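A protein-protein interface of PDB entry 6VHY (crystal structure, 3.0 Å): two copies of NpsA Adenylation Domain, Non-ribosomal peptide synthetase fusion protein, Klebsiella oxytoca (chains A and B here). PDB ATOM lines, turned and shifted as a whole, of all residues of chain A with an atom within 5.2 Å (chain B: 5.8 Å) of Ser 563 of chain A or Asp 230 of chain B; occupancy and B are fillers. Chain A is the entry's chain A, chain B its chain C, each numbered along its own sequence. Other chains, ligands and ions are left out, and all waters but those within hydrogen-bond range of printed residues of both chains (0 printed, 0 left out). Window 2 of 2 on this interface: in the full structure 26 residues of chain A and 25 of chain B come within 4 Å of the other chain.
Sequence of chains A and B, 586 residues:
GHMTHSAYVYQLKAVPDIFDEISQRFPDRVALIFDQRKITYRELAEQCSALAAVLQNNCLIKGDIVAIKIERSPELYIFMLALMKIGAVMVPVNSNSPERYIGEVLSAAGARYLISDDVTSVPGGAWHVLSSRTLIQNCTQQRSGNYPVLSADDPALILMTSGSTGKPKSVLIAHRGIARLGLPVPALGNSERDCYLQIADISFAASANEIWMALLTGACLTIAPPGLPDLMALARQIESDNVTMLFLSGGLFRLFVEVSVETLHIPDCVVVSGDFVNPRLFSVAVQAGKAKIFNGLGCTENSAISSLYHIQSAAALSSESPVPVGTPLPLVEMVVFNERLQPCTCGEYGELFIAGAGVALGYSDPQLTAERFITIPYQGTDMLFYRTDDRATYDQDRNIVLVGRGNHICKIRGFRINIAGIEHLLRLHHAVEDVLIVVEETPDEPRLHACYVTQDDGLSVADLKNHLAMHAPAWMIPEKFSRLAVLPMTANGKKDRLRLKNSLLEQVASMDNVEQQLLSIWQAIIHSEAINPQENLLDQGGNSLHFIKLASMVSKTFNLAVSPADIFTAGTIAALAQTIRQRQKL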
ATOM      1  N   ILE A 548      20.970 -32.055 -17.568  1.00  0.00           N
ATOM      2  CA  ILE A 548      20.517 -30.714 -17.207  1.00  0.00           C
ATOM      3  C   ILE A 548      19.293 -30.779 -16.303  1.00  0.00           C
ATOM      4  O   ILE A 548      19.217 -30.086 -15.283  1.00  0.00           O
ATOM      5  CB  ILE A 548      20.228 -29.888 -18.472  1.00  0.00           C
ATOM      6  CG1 ILE A 548      21.503 -29.694 -19.286  1.00  0.00           C
ATOM      7  CG2 ILE A 548      19.641 -28.541 -18.102  1.00  0.00           C
ATOM      8  CD1 ILE A 548      21.260 -29.055 -20.623  1.00  0.00           C
ATOM      9  N   ALA A 551      20.420 -31.930 -12.728  1.00  0.00           N
ATOM     10  CA  ALA A 551      21.089 -30.909 -11.929  1.00  0.00           C
ATOM     11  C   ALA A 551      20.124 -29.826 -11.462  1.00  0.00           C
ATOM     12  O   ALA A 551      20.236 -29.340 -10.331  1.00  0.00           O
ATOM     13  CB  ALA A 551      22.236 -30.293 -12.727  1.00  0.00           C
ATOM     14  N   SER A 555      18.907 -28.886  -7.546  1.00  0.00           N
ATOM     15  CA  SER A 555      18.968 -27.529  -7.023  1.00  0.00           C
ATOM     16  C   SER A 555      17.598 -27.071  -6.548  1.00  0.00           C
ATOM     17  O   SER A 555      17.496 -26.271  -5.612  1.00  0.00           O
ATOM     18  CB  SER A 555      19.512 -26.579  -8.090  1.00  0.00           C
ATOM     19  OG  SER A 555      20.809 -26.968  -8.502  1.00  0.00           O
ATOM     20  N   ALA A 561      22.970 -24.433  -5.258  1.00  0.00           N
ATOM     21  CA  ALA A 561      23.231 -24.325  -6.689  1.00  0.00           C
ATOM     22  C   ALA A 561      24.052 -25.531  -7.121  1.00  0.00           C
ATOM     23  O   ALA A 561      25.202 -25.698  -6.702  1.00  0.00           O
ATOM     24  CB  ALA A 561      23.955 -23.022  -7.004  1.00  0.00           C
ATOM     25  N   VAL A 562      23.459 -26.373  -7.962  1.00  0.00           N
ATOM     26  CA  VAL A 562      24.119 -27.543  -8.523  1.00  0.00           C
ATOM     27  C   VAL A 562      24.114 -27.392 -10.034  1.00  0.00           C
ATOM     28  O   VAL A 562      23.050 -27.244 -10.644  1.00  0.00           O
ATOM     29  CB  VAL A 562      23.425 -28.846  -8.100  1.00  0.00           C
ATOM     30  CG1 VAL A 562      24.069 -30.041  -8.779  1.00  0.00           C
ATOM     31  CG2 VAL A 562      23.466 -28.993  -6.593  1.00  0.00           C
ATOM     32  N   SER A 563      25.287 -27.443 -10.630  1.00  0.00           N
ATOM     33  CA  SER A 563      25.408 -27.334 -12.070  1.00  0.00           C
ATOM     34  C   SER A 563      25.655 -28.699 -12.686  1.00  0.00           C
ATOM     35  O   SER A 563      26.002 -29.654 -11.985  1.00  0.00           O
ATOM     36  CB  SER A 563      26.558 -26.386 -12.426  1.00  0.00           C
ATOM     37  OG  SER A 563      27.805 -26.927 -12.030  1.00  0.00           O
ATOM     38  N   PRO A 564      25.472 -28.839 -14.003  1.00  0.00           N
ATOM     39  CA  PRO A 564      25.875 -30.093 -14.655  1.00  0.00           C
ATOM     40  C   PRO A 564      27.339 -30.415 -14.442  1.00  0.00           C
ATOM     41  O   PRO A 564      27.717 -31.593 -14.445  1.00  0.00           O
ATOM     42  CB  PRO A 564      25.550 -29.839 -16.130  1.00  0.00           C
ATOM     43  CG  PRO A 564      24.459 -28.830 -16.097  1.00  0.00           C
ATOM     44  CD  PRO A 564      24.764 -27.942 -14.931  1.00  0.00           C
ATOM     45  N   ALA A 565      28.177 -29.394 -14.268  1.00  0.00           N
ATOM     46  CA  ALA A 565      29.584 -29.632 -13.971  1.00  0.00           C
ATOM     47  C   ALA A 565      29.741 -30.277 -12.602  1.00  0.00           C
ATOM     48  O   ALA A 565      30.597 -31.148 -12.411  1.00  0.00           O
ATOM     49  CB  ALA A 565      30.369 -28.325 -14.046  1.00  0.00           C
ATOM     50  N   ASP A 566      28.918 -29.858 -11.639  1.00  0.00           N
ATOM     51  CA  ASP A 566      28.945 -30.469 -10.316  1.00  0.00           C
ATOM     52  C   ASP A 566      28.525 -31.930 -10.379  1.00  0.00           C
ATOM     53  O   ASP A 566      29.064 -32.770  -9.649  1.00  0.00           O
ATOM     54  CB  ASP A 566      28.033 -29.694  -9.367  1.00  0.00           C
ATOM     55  CG  ASP A 566      28.456 -28.250  -9.206  1.00  0.00           C
ATOM     56  OD1 ASP A 566      29.611 -28.007  -8.802  1.00  0.00           O
ATOM     57  OD2 ASP A 566      27.632 -27.356  -9.492  1.00  0.00           O
ATOM     58  N   ILE A 567      27.556 -32.253 -11.238  1.00  0.00           N
ATOM     59  CA  ILE A 567      27.142 -33.643 -11.393  1.00  0.00           C
ATOM     60  C   ILE A 567      28.264 -34.468 -12.011  1.00  0.00           C
ATOM     61  O   ILE A 567      28.534 -35.594 -11.579  1.00  0.00           O
ATOM     62  CB  ILE A 567      25.851 -33.729 -12.226  1.00  0.00           C
ATOM     63  N   LEU B 228      27.639 -26.700 -21.306  1.00  0.00           N
ATOM     64  CA  LEU B 228      26.241 -27.080 -21.245  1.00  0.00           C
ATOM     65  C   LEU B 228      25.429 -25.990 -20.550  1.00  0.00           C
ATOM     66  O   LEU B 228      25.915 -25.338 -19.623  1.00  0.00           O
ATOM     67  CB  LEU B 228      26.075 -28.406 -20.511  1.00  0.00           C
ATOM     68  CG  LEU B 228      26.518 -29.625 -21.319  1.00  0.00           C
ATOM     69  CD1 LEU B 228      27.951 -29.995 -20.968  1.00  0.00           C
ATOM     70  CD2 LEU B 228      25.584 -30.799 -21.102  1.00  0.00           C
ATOM     71  N   PRO B 229      24.189 -25.779 -20.979  1.00  0.00           N
ATOM     72  CA  PRO B 229      23.286 -24.902 -20.227  1.00  0.00           C
ATOM     73  C   PRO B 229      23.020 -25.411 -18.819  1.00  0.00           C
ATOM     74  O   PRO B 229      22.815 -26.604 -18.593  1.00  0.00           O
ATOM     75  CB  PRO B 229      22.009 -24.906 -21.072  1.00  0.00           C
ATOM     76  CG  PRO B 229      22.461 -25.253 -22.434  1.00  0.00           C
ATOM     77  CD  PRO B 229      23.613 -26.193 -22.265  1.00  0.00           C
ATOM     78  N   ASP B 230      23.027 -24.480 -17.871  1.00  0.00           N
ATOM     79  CA  ASP B 230      22.652 -24.727 -16.485  1.00  0.00           C
ATOM     80  C   ASP B 230      21.294 -24.065 -16.289  1.00  0.00           C
ATOM     81  O   ASP B 230      21.209 -22.836 -16.191  1.00  0.00           O
ATOM     82  CB  ASP B 230      23.698 -24.170 -15.521  1.00  0.00           C
ATOM     83  CG  ASP B 230      23.355 -24.424 -14.061  1.00  0.00           C
ATOM     84  OD1 ASP B 230      22.329 -25.079 -13.782  1.00  0.00           O
ATOM     85  OD2 ASP B 230      24.115 -23.960 -13.187  1.00  0.00           O
ATOM     86  N   LEU B 231      20.240 -24.881 -16.228  1.00  0.00           N
ATOM     87  CA  LEU B 231      18.880 -24.356 -16.309  1.00  0.00           C
ATOM     88  C   LEU B 231      18.604 -23.328 -15.221  1.00  0.00           C
ATOM     89  O   LEU B 231      17.884 -22.351 -15.450  1.00  0.00           O
ATOM     90  CB  LEU B 231      17.881 -25.505 -16.213  1.00  0.00           C
ATOM     91  CG  LEU B 231      16.495 -25.261 -16.797  1.00  0.00           C
ATOM     92  CD1 LEU B 231      16.602 -25.179 -18.296  1.00  0.00           C
ATOM     93  CD2 LEU B 231      15.538 -26.358 -16.400  1.00  0.00           C
ATOM     94  N   MET B 232      19.162 -23.530 -14.032  1.00  0.00           N
ATOM     95  CA  MET B 232      18.974 -22.570 -12.953  1.00  0.00           C
ATOM     96  C   MET B 232      19.848 -21.336 -13.128  1.00  0.00           C
ATOM     97  O   MET B 232      19.416 -20.220 -12.822  1.00  0.00           O
ATOM     98  CB  MET B 232      19.257 -23.235 -11.607  1.00  0.00           C
ATOM     99  CG  MET B 232      18.293 -24.349 -11.239  1.00  0.00           C
ATOM    100  SD  MET B 232      16.591 -23.768 -11.135  1.00  0.00           S
ATOM    101  CE  MET B 232      15.854 -24.604 -12.530  1.00  0.00           C
ATOM    102  N   ALA B 233      21.071 -21.514 -13.621  1.00  0.00           N
ATOM    103  CA  ALA B 233      21.892 -20.361 -13.968  1.00  0.00           C
ATOM    104  C   ALA B 233      21.256 -19.545 -15.084  1.00  0.00           C
ATOM    105  O   ALA B 233      21.336 -18.312 -15.081  1.00  0.00           O
ATOM    106  CB  ALA B 233      23.295 -20.814 -14.364  1.00  0.00           C
ATOM    107  N   LEU B 234      20.621 -20.212 -16.046  1.00  0.00           N
ATOM    108  CA  LEU B 234      19.930 -19.484 -17.102  1.00  0.00           C
ATOM    109  C   LEU B 234      18.746 -18.700 -16.555  1.00  0.00           C
ATOM    110  O   LEU B 234      18.522 -17.552 -16.949  1.00  0.00           O
ATOM    111  CB  LEU B 234      19.475 -20.456 -18.185  1.00  0.00           C
ATOM    112  CG  LEU B 234      20.584 -21.026 -19.064  1.00  0.00           C
ATOM    113  CD1 LEU B 234      19.998 -21.927 -20.123  1.00  0.00           C
ATOM    114  CD2 LEU B 234      21.385 -19.914 -19.692  1.00  0.00           C
ATOM    115  N   ALA B 235      17.981 -19.298 -15.639  1.00  0.00           N
ATOM    116  CA  ALA B 235      16.887 -18.568 -15.009  1.00  0.00           C
ATOM    117  C   ALA B 235      17.424 -17.359 -14.262  1.00  0.00           C
ATOM    118  O   ALA B 235      16.889 -16.252 -14.375  1.00  0.00           O
ATOM    119  CB  ALA B 235      16.110 -19.488 -14.073  1.00  0.00           C
ATOM    120  N   ARG B 236      18.491 -17.591 -13.523  1.00  0.00           N
ATOM    121  CA  ARG B 236      19.121 -16.500 -12.757  1.00  0.00           C
ATOM    122  C   ARG B 236      19.553 -15.431 -13.745  1.00  0.00           C
ATOM    123  O   ARG B 236      19.289 -14.269 -13.494  1.00  0.00           O
ATOM    124  CB  ARG B 236      20.403 -17.015 -12.106  1.00  0.00           C
ATOM    125  CG  ARG B 236      20.396 -17.047 -10.586  1.00  0.00           C
ATOM    126  CD  ARG B 236      21.806 -17.126 -10.040  1.00  0.00           C
ATOM    127  NE  ARG B 236      22.462 -18.361 -10.427  1.00  0.00           N
ATOM    128  CZ  ARG B 236      21.955 -19.565 -10.233  1.00  0.00           C
ATOM    129  NH1 ARG B 236      20.703 -19.698  -9.845  1.00  0.00           N
ATOM    130  NH2 ARG B 236      22.696 -20.635 -10.422  1.00  0.00           N
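The side-chain hydroxyl (OG) of Ser 555 of chain A sits at hydrogen-bond distance from the backbone NH (N) of Val 562 of chain A. OG of Ser 563 of chain A lies close to N of Ala 565 of chain A (3.4 Å). The side-chain carboxylate of Asp 566 of chain A is in hydrogen-bond range of the side-chain hydroxyl of Ser 563 of chain A, 2.6 Å away.
Among the printed residues, pairs that only touch across the chains: Ile 548 of chain A with Pro 229 of chain B, Ser 563 of chain A with Asp 230 of chain B, Pro 564 of chain A with Pro 229 of chain B, Val 562 of chain A with Asp 230 of chain B, Pro 564 of chain A with Asp 230 of chain B and Ile 548 of chain A with Leu 231 of chain B.
Of the printed residues of chain A, Asp 230 of chain B touches Val 562, Ser 563 and Pro 564. Of the printed residues of chain A, Leu 231 of chain B touches Ile 548. Printed residues of chain B within 4 Å of Pro 564 of chain A: Pro 229 and Asp 230. Of the printed residues of chain B, Ile 548 of chain A touches Pro 229 (3.4 Å) and Leu 231 (3.99 Å). Printed residues of chain A within 4 Å of Pro 229 of chain B: Ile 548 (3.4 Å) and Pro 564 (3.7 Å). The nearest residue of chain A that does not touch Asp 230 of chain B is Ile 548 of chain A (5.1 Å).
Printed residues of chain A that touch a printed residue of chain B: Ile 548, Val 562, Ser 563 and Pro 564. Hydrophobic or aromatic side chains of chain B within 4 Å of the printed part of chain A: Leu 231. Among the printed residues, 6 pairs touch across the chains. Among the printed residues, no Asp or Glu carboxylate lies within 4 Å of a Lys or Arg side-chain nitrogen of the other chain.
No position is printed for both chains.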
